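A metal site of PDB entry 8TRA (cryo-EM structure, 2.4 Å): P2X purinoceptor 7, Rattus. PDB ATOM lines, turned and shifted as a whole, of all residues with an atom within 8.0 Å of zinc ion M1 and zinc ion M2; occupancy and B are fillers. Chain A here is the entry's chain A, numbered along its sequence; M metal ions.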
ATOM      1  N   VAL A 404      -8.945  16.217  24.512  1.00  0.00           N
ATOM      2  CA  VAL A 404     -10.376  16.206  24.205  1.00  0.00           C
ATOM      3  C   VAL A 404     -10.606  15.909  22.736  1.00  0.00           C
ATOM      4  O   VAL A 404     -11.559  15.199  22.376  1.00  0.00           O
ATOM      5  CB  VAL A 404     -11.018  17.545  24.629  1.00  0.00           C
ATOM      6  CG1 VAL A 404     -10.656  18.651  23.640  1.00  0.00           C
ATOM      7  CG2 VAL A 404     -12.531  17.394  24.741  1.00  0.00           C
ATOM      8  N   GLN A 422       3.516  18.052  26.322  1.00  0.00           N
ATOM      9  CA  GLN A 422       2.680  18.127  25.135  1.00  0.00           C
ATOM     10  C   GLN A 422       3.428  17.664  23.893  1.00  0.00           C
ATOM     11  O   GLN A 422       2.886  16.937  23.057  1.00  0.00           O
ATOM     12  CB  GLN A 422       2.156  19.549  24.955  1.00  0.00           C
ATOM     13  CG  GLN A 422       1.108  19.700  23.863  1.00  0.00           C
ATOM     14  CD  GLN A 422      -0.317  19.565  24.381  1.00  0.00           C
ATOM     15  OE1 GLN A 422      -0.532  19.389  25.582  1.00  0.00           O
ATOM     16  NE2 GLN A 422      -1.285  19.646  23.486  1.00  0.00           N
ATOM     17  N   SER A 473      -1.113  33.133  24.920  1.00  0.00           N
ATOM     18  CA  SER A 473      -1.011  31.798  25.493  1.00  0.00           C
ATOM     19  C   SER A 473       0.350  31.188  25.164  1.00  0.00           C
ATOM     20  O   SER A 473       0.989  31.558  24.177  1.00  0.00           O
ATOM     21  CB  SER A 473      -2.133  30.909  24.976  1.00  0.00           C
ATOM     22  OG  SER A 473      -1.896  30.525  23.623  1.00  0.00           O
ATOM     23  N   PRO A 474       0.815  30.235  25.974  1.00  0.00           N
ATOM     24  CA  PRO A 474       2.089  29.586  25.683  1.00  0.00           C
ATOM     25  C   PRO A 474       2.108  28.954  24.299  1.00  0.00           C
ATOM     26  O   PRO A 474       1.065  28.729  23.665  1.00  0.00           O
ATOM     27  CB  PRO A 474       2.209  28.514  26.785  1.00  0.00           C
ATOM     28  CG  PRO A 474       1.353  28.999  27.890  1.00  0.00           C
ATOM     29  CD  PRO A 474       0.257  29.835  27.281  1.00  0.00           C
ATOM     30  N   TRP A 476       2.974  25.899  23.447  1.00  0.00           N
ATOM     31  CA  TRP A 476       2.427  24.549  23.447  1.00  0.00           C
ATOM     32  C   TRP A 476       0.917  24.512  23.689  1.00  0.00           C
ATOM     33  O   TRP A 476       0.300  23.474  23.468  1.00  0.00           O
ATOM     34  CB  TRP A 476       3.124  23.677  24.505  1.00  0.00           C
ATOM     35  CG  TRP A 476       3.263  24.324  25.852  1.00  0.00           C
ATOM     36  CD1 TRP A 476       4.376  24.902  26.370  1.00  0.00           C
ATOM     37  CD2 TRP A 476       2.240  24.444  26.850  1.00  0.00           C
ATOM     38  NE1 TRP A 476       4.119  25.378  27.628  1.00  0.00           N
ATOM     39  CE2 TRP A 476       2.818  25.113  27.952  1.00  0.00           C
ATOM     40  CE3 TRP A 476       0.904  24.065  26.926  1.00  0.00           C
ATOM     41  CZ2 TRP A 476       2.098  25.407  29.103  1.00  0.00           C
ATOM     42  CZ3 TRP A 476       0.190  24.351  28.077  1.00  0.00           C
ATOM     43  CH2 TRP A 476       0.788  25.012  29.151  1.00  0.00           C
ATOM     44  N   CYS A 477       0.327  25.616  24.134  1.00  0.00           N
ATOM     45  CA  CYS A 477      -1.110  25.653  24.391  1.00  0.00           C
ATOM     46  C   CYS A 477      -1.881  25.796  23.084  1.00  0.00           C
ATOM     47  O   CYS A 477      -1.495  26.556  22.197  1.00  0.00           O
ATOM     48  CB  CYS A 477      -1.456  26.801  25.333  1.00  0.00           C
ATOM     49  SG  CYS A 477      -3.228  27.033  25.580  1.00  0.00           S
ATOM     50  N   GLN A 478      -2.995  25.060  22.989  1.00  0.00           N
ATOM     51  CA  GLN A 478      -3.885  25.120  21.834  1.00  0.00           C
ATOM     52  C   GLN A 478      -5.313  25.444  22.245  1.00  0.00           C
ATOM     53  O   GLN A 478      -6.252  25.192  21.482  1.00  0.00           O
ATOM     54  CB  GLN A 478      -3.829  23.803  21.056  1.00  0.00           C
ATOM     55  CG  GLN A 478      -2.738  23.737  20.003  1.00  0.00           C
ATOM     56  CD  GLN A 478      -1.601  22.799  20.400  1.00  0.00           C
ATOM     57  OE1 GLN A 478      -1.835  21.743  20.981  1.00  0.00           O
ATOM     58  NE2 GLN A 478      -0.376  23.183  20.072  1.00  0.00           N
ATOM     59  N   CYS A 479      -5.507  26.006  23.434  1.00  0.00           N
ATOM     60  CA  CYS A 479      -6.837  26.329  23.939  1.00  0.00           C
ATOM     61  C   CYS A 479      -6.984  27.750  24.464  1.00  0.00           C
ATOM     62  O   CYS A 479      -8.115  28.203  24.640  1.00  0.00           O
ATOM     63  CB  CYS A 479      -7.234  25.349  25.049  1.00  0.00           C
ATOM     64  SG  CYS A 479      -6.606  25.776  26.688  1.00  0.00           S
ATOM     65  N   GLY A 480      -5.887  28.461  24.708  1.00  0.00           N
ATOM     66  CA  GLY A 480      -5.951  29.849  25.133  1.00  0.00           C
ATOM     67  C   GLY A 480      -6.222  30.065  26.601  1.00  0.00           C
ATOM     68  O   GLY A 480      -6.362  31.216  27.028  1.00  0.00           O
ATOM     69  N   ASN A 481      -6.299  28.991  27.398  1.00  0.00           N
ATOM     70  CA  ASN A 481      -6.571  29.111  28.827  1.00  0.00           C
ATOM     71  C   ASN A 481      -5.437  28.573  29.696  1.00  0.00           C
ATOM     72  O   ASN A 481      -5.501  28.696  30.923  1.00  0.00           O
ATOM     73  CB  ASN A 481      -7.870  28.380  29.185  1.00  0.00           C
ATOM     74  CG  ASN A 481      -9.067  28.924  28.445  1.00  0.00           C
ATOM     75  OD1 ASN A 481      -9.586  28.306  27.519  1.00  0.00           O
ATOM     76  ND2 ASN A 481      -9.525  30.112  28.851  1.00  0.00           N
ATOM     77  N   CYS A 482      -4.411  27.970  29.099  1.00  0.00           N
ATOM     78  CA  CYS A 482      -3.294  27.442  29.864  1.00  0.00           C
ATOM     79  C   CYS A 482      -2.355  28.566  30.278  1.00  0.00           C
ATOM     80  O   CYS A 482      -2.307  29.641  29.674  1.00  0.00           O
ATOM     81  CB  CYS A 482      -2.538  26.398  29.050  1.00  0.00           C
ATOM     82  SG  CYS A 482      -3.482  24.896  28.711  1.00  0.00           S
ATOM     83  N   LEU A 483      -1.589  28.306  31.338  1.00  0.00           N
ATOM     84  CA  LEU A 483      -0.633  29.247  31.895  1.00  0.00           C
ATOM     85  C   LEU A 483       0.692  28.552  32.141  1.00  0.00           C
ATOM     86  O   LEU A 483       0.737  27.324  32.287  1.00  0.00           O
ATOM     87  CB  LEU A 483      -1.160  29.835  33.208  1.00  0.00           C
ATOM     88  CG  LEU A 483      -2.574  30.426  33.172  1.00  0.00           C
ATOM     89  CD1 LEU A 483      -3.084  30.675  34.579  1.00  0.00           C
ATOM     90  CD2 LEU A 483      -2.592  31.705  32.353  1.00  0.00           C
ATOM     91  N   LEU A 497       1.308  21.045  29.594  1.00  0.00           N
ATOM     92  CA  LEU A 497       0.373  20.204  28.874  1.00  0.00           C
ATOM     93  C   LEU A 497      -0.924  20.966  28.649  1.00  0.00           C
ATOM     94  O   LEU A 497      -1.395  21.689  29.534  1.00  0.00           O
ATOM     95  CB  LEU A 497       0.088  18.913  29.652  1.00  0.00           C
ATOM     96  CG  LEU A 497      -0.919  17.926  29.057  1.00  0.00           C
ATOM     97  CD1 LEU A 497      -0.269  17.088  27.977  1.00  0.00           C
ATOM     98  CD2 LEU A 497      -1.504  17.047  30.152  1.00  0.00           C
ATOM     99  N   CYS A 498      -1.490  20.815  27.457  1.00  0.00           N
ATOM    100  CA  CYS A 498      -2.749  21.445  27.080  1.00  0.00           C
ATOM    101  C   CYS A 498      -3.848  20.391  26.969  1.00  0.00           C
ATOM    102  O   CYS A 498      -3.577  19.195  26.857  1.00  0.00           O
ATOM    103  CB  CYS A 498      -2.610  22.202  25.755  1.00  0.00           C
ATOM    104  SG  CYS A 498      -4.018  23.279  25.368  1.00  0.00           S
ATOM    105  N   CYS A 499      -5.087  20.866  27.008  1.00  0.00           N
ATOM    106  CA  CYS A 499      -6.242  19.966  26.934  1.00  0.00           C
ATOM    107  C   CYS A 499      -6.445  19.363  25.549  1.00  0.00           C
ATOM    108  O   CYS A 499      -7.245  18.433  25.419  1.00  0.00           O
ATOM    109  CB  CYS A 499      -7.504  20.712  27.344  1.00  0.00           C
ATOM    110  SG  CYS A 499      -7.856  22.187  26.354  1.00  0.00           S
ATOM    111  N   ARG A 500      -5.733  19.848  24.528  1.00  0.00           N
ATOM    112  CA  ARG A 500      -5.931  19.367  23.175  1.00  0.00           C
ATOM    113  C   ARG A 500      -4.625  19.464  22.405  1.00  0.00           C
ATOM    114  O   ARG A 500      -3.702  20.190  22.783  1.00  0.00           O
ATOM    115  CB  ARG A 500      -7.019  20.170  22.450  1.00  0.00           C
ATOM    116  CG  ARG A 500      -6.945  21.672  22.668  1.00  0.00           C
ATOM    117  CD  ARG A 500      -8.145  22.386  22.073  1.00  0.00           C
ATOM    118  NE  ARG A 500      -8.688  21.685  20.911  1.00  0.00           N
ATOM    119  CZ  ARG A 500      -9.977  21.462  20.686  1.00  0.00           C
ATOM    120  NH1 ARG A 500     -10.916  21.899  21.516  1.00  0.00           N
ATOM    121  NH2 ARG A 500     -10.338  20.784  19.606  1.00  0.00           N
ATOM    122  N   GLY A 504      -8.520  24.936  19.269  1.00  0.00           N
ATOM    123  CA  GLY A 504      -9.949  24.744  19.411  1.00  0.00           C
ATOM    124  C   GLY A 504     -10.430  25.264  20.741  1.00  0.00           C
ATOM    125  O   GLY A 504      -9.745  26.031  21.412  1.00  0.00           O
ATOM    126  N   GLN A 505     -11.633  24.830  21.123  1.00  0.00           N
ATOM    127  CA  GLN A 505     -12.240  25.269  22.371  1.00  0.00           C
ATOM    128  C   GLN A 505     -11.737  24.424  23.537  1.00  0.00           C
ATOM    129  O   GLN A 505     -11.594  23.200  23.421  1.00  0.00           O
ATOM    130  CB  GLN A 505     -13.767  25.186  22.283  1.00  0.00           C
ATOM    131  CG  GLN A 505     -14.297  23.882  21.722  1.00  0.00           C
ATOM    132  CD  GLN A 505     -15.760  23.650  22.065  1.00  0.00           C
ATOM    133  OE1 GLN A 505     -16.310  24.278  22.972  1.00  0.00           O
ATOM    134  NE2 GLN A 505     -16.400  22.747  21.336  1.00  0.00           N
ATOM    135  N   CYS A 506     -11.474  25.079  24.655  1.00  0.00           N
ATOM    136  CA  CYS A 506     -10.985  24.394  25.842  1.00  0.00           C
ATOM    137  C   CYS A 506     -12.058  23.484  26.428  1.00  0.00           C
ATOM    138  O   CYS A 506     -13.257  23.766  26.334  1.00  0.00           O
ATOM    139  CB  CYS A 506     -10.522  25.402  26.895  1.00  0.00           C
ATOM    140  SG  CYS A 506      -9.856  24.667  28.403  1.00  0.00           S
ATOM    141  N   ILE A 507     -11.612  22.389  27.032  1.00  0.00           N
ATOM    142  CA  ILE A 507     -12.540  21.465  27.676  1.00  0.00           C
ATOM    143  C   ILE A 507     -13.265  22.147  28.830  1.00  0.00           C
ATOM    144  O   ILE A 507     -14.382  21.751  29.196  1.00  0.00           O
ATOM    145  CB  ILE A 507     -11.800  20.195  28.151  1.00  0.00           C
ATOM    146  CG1 ILE A 507     -12.804  19.126  28.578  1.00  0.00           C
ATOM    147  CG2 ILE A 507     -10.858  20.528  29.297  1.00  0.00           C
ATOM    148  CD1 ILE A 507     -12.189  17.756  28.748  1.00  0.00           C
ATOM    149  N   THR A 508     -12.646  23.168  29.418  1.00  0.00           N
ATOM    150  CA  THR A 508     -13.274  23.873  30.533  1.00  0.00           C
ATOM    151  C   THR A 508     -14.582  24.534  30.103  1.00  0.00           C
ATOM    152  O   THR A 508     -15.476  24.732  30.936  1.00  0.00           O
ATOM    153  CB  THR A 508     -12.331  24.927  31.097  1.00  0.00           C
ATOM    154  OG1 THR A 508     -11.964  25.856  30.071  1.00  0.00           O
ATOM    155  CG2 THR A 508     -11.070  24.271  31.661  1.00  0.00           C
ATOM    156  N   THR A 509     -14.717  24.876  28.816  1.00  0.00           N
ATOM    157  CA  THR A 509     -15.933  25.531  28.345  1.00  0.00           C
ATOM    158  C   THR A 509     -17.158  24.626  28.479  1.00  0.00           C
ATOM    159  O   THR A 509     -18.279  25.144  28.555  1.00  0.00           O
ATOM    160  CB  THR A 509     -15.769  25.950  26.885  1.00  0.00           C
ATOM    161  OG1 THR A 509     -15.621  24.800  26.057  1.00  0.00           O
ATOM    162  CG2 THR A 509     -14.545  26.844  26.731  1.00  0.00           C
ATOM    163  N   PHE A 513     -17.612  20.200  32.889  1.00  0.00           N
ATOM    164  CA  PHE A 513     -16.445  20.574  33.680  1.00  0.00           C
ATOM    165  C   PHE A 513     -16.850  21.285  34.963  1.00  0.00           C
ATOM    166  O   PHE A 513     -16.328  20.987  36.040  1.00  0.00           O
ATOM    167  CB  PHE A 513     -15.501  21.449  32.855  1.00  0.00           C
ATOM    168  CG  PHE A 513     -14.185  21.717  33.514  1.00  0.00           C
ATOM    169  CD1 PHE A 513     -14.054  22.748  34.435  1.00  0.00           C
ATOM    170  CD2 PHE A 513     -13.082  20.933  33.242  1.00  0.00           C
ATOM    171  CE1 PHE A 513     -12.840  22.997  35.047  1.00  0.00           C
ATOM    172  CE2 PHE A 513     -11.871  21.181  33.845  1.00  0.00           C
ATOM    173  CZ  PHE A 513     -11.744  22.211  34.756  1.00  0.00           C
ATOM    174  N   TYR A 553     -11.664  15.046  37.746  1.00  0.00           N
ATOM    175  CA  TYR A 553     -11.253  15.215  36.358  1.00  0.00           C
ATOM    176  C   TYR A 553     -10.510  13.978  35.860  1.00  0.00           C
ATOM    177  O   TYR A 553     -10.736  13.521  34.737  1.00  0.00           O
ATOM    178  CB  TYR A 553     -10.382  16.461  36.207  1.00  0.00           C
ATOM    179  CG  TYR A 553      -9.825  16.624  34.811  1.00  0.00           C
ATOM    180  CD1 TYR A 553     -10.520  17.307  33.827  1.00  0.00           C
ATOM    181  CD2 TYR A 553      -8.589  16.086  34.472  1.00  0.00           C
ATOM    182  CE1 TYR A 553     -10.014  17.460  32.558  1.00  0.00           C
ATOM    183  CE2 TYR A 553      -8.071  16.223  33.202  1.00  0.00           C
ATOM    184  CZ  TYR A 553      -8.787  16.914  32.245  1.00  0.00           C
ATOM    185  OH  TYR A 553      -8.283  17.053  30.980  1.00  0.00           O
ATOM    186  N   PRO A 570      -4.299  18.935  32.495  1.00  0.00           N
ATOM    187  CA  PRO A 570      -3.865  20.055  31.650  1.00  0.00           C
ATOM    188  C   PRO A 570      -3.703  21.324  32.477  1.00  0.00           C
ATOM    189  O   PRO A 570      -4.336  21.504  33.521  1.00  0.00           O
ATOM    190  CB  PRO A 570      -4.993  20.194  30.621  1.00  0.00           C
ATOM    191  CG  PRO A 570      -5.704  18.886  30.651  1.00  0.00           C
ATOM    192  CD  PRO A 570      -5.588  18.387  32.046  1.00  0.00           C
ATOM    193  N   SER A 571      -2.840  22.214  31.980  1.00  0.00           N
ATOM    194  CA  SER A 571      -2.590  23.455  32.694  1.00  0.00           C
ATOM    195  C   SER A 571      -3.855  24.283  32.834  1.00  0.00           C
ATOM    196  O   SER A 571      -4.105  24.877  33.898  1.00  0.00           O
ATOM    197  CB  SER A 571      -1.503  24.263  31.980  1.00  0.00           C
ATOM    198  OG  SER A 571      -1.202  25.457  32.674  1.00  0.00           O
ATOM    199  N   CYS A 572      -4.675  24.334  31.784  1.00  0.00           N
ATOM    200  CA  CYS A 572      -5.906  25.119  31.844  1.00  0.00           C
ATOM    201  C   CYS A 572      -6.817  24.622  32.960  1.00  0.00           C
ATOM    202  O   CYS A 572      -7.256  25.406  33.812  1.00  0.00           O
ATOM    203  CB  CYS A 572      -6.632  25.052  30.502  1.00  0.00           C
ATOM    204  SG  CYS A 572      -6.486  23.449  29.664  1.00  0.00           S
ATOM    205  N   CYS A 573      -7.107  23.315  32.979  1.00  0.00           N
ATOM    206  CA  CYS A 573      -7.995  22.770  33.987  1.00  0.00           C
ATOM    207  C   CYS A 573      -7.385  22.862  35.377  1.00  0.00           C
ATOM    208  O   CYS A 573      -8.066  23.186  36.349  1.00  0.00           O
ATOM    209  CB  CYS A 573      -8.337  21.322  33.651  1.00  0.00           C
ATOM    210  SG  CYS A 573      -8.795  21.058  31.924  1.00  0.00           S
HETATM  211 ZN    ZN M   1      -7.701  24.026  27.766  1.00  0.00          ZN
HETATM  212 ZN    ZN M   2      -4.344  25.240  26.575  1.00  0.00          ZN
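SG of Cys 499 is bound to zinc ion M1 (2.3 Å). SG of Cys 572 is bound to zinc ion M1, at 2.3 Å. The side-chain sulfur (SG) of Cys 479 is bound to zinc ion M1 (2.3 Å). The side-chain sulfur (SG) of Cys 506 binds zinc ion M1 (2.3 Å).
The backbone NH (N) of Val 404 sits at hydrogen-bond distance from the backbone carbonyl oxygen (O) of Cys 499 (2.9 Å). The side-chain amide oxygen (OE1) of Gln 422 is in hydrogen-bond range of the backbone NH (N) of Cys 498 (2.5 Å). The side-chain amide oxygen (OD1) of Asn 481 lies close to the backbone carbonyl oxygen (O) of Cys 479, 3.2 Å away. The side-chain sulfur (SG) of Cys 477 sits close to the backbone NH (N) of Gly 480 (3.1 Å). OG1 of Thr 508 sits close to SG of Cys 506 (2.9 Å). The side-chain amide nitrogen of Gln 478 lies within hydrogen-bond range of the backbone carbonyl oxygen of Trp 476 (3.5 Å). O of Gln 478 lies within hydrogen-bond range of N of Gly 504 (3.2 Å). OE1 of Gln 478 lies within hydrogen-bond range of NE2 of Gln 422 (3.3 Å).
Gln 478 touches zinc ion M2 (N to ZN, 3.8 Å).
Zinc ion M2 is bound by SG of Cys 498, SG of Cys 479, SG of Cys 482 and SG of Cys 477.
Of the 28 residues printed, 4 come within 4 Å of zinc ion M1. The nearest printed residue that does not touch zinc ion M1 is Ile 507 (4.3 Å).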
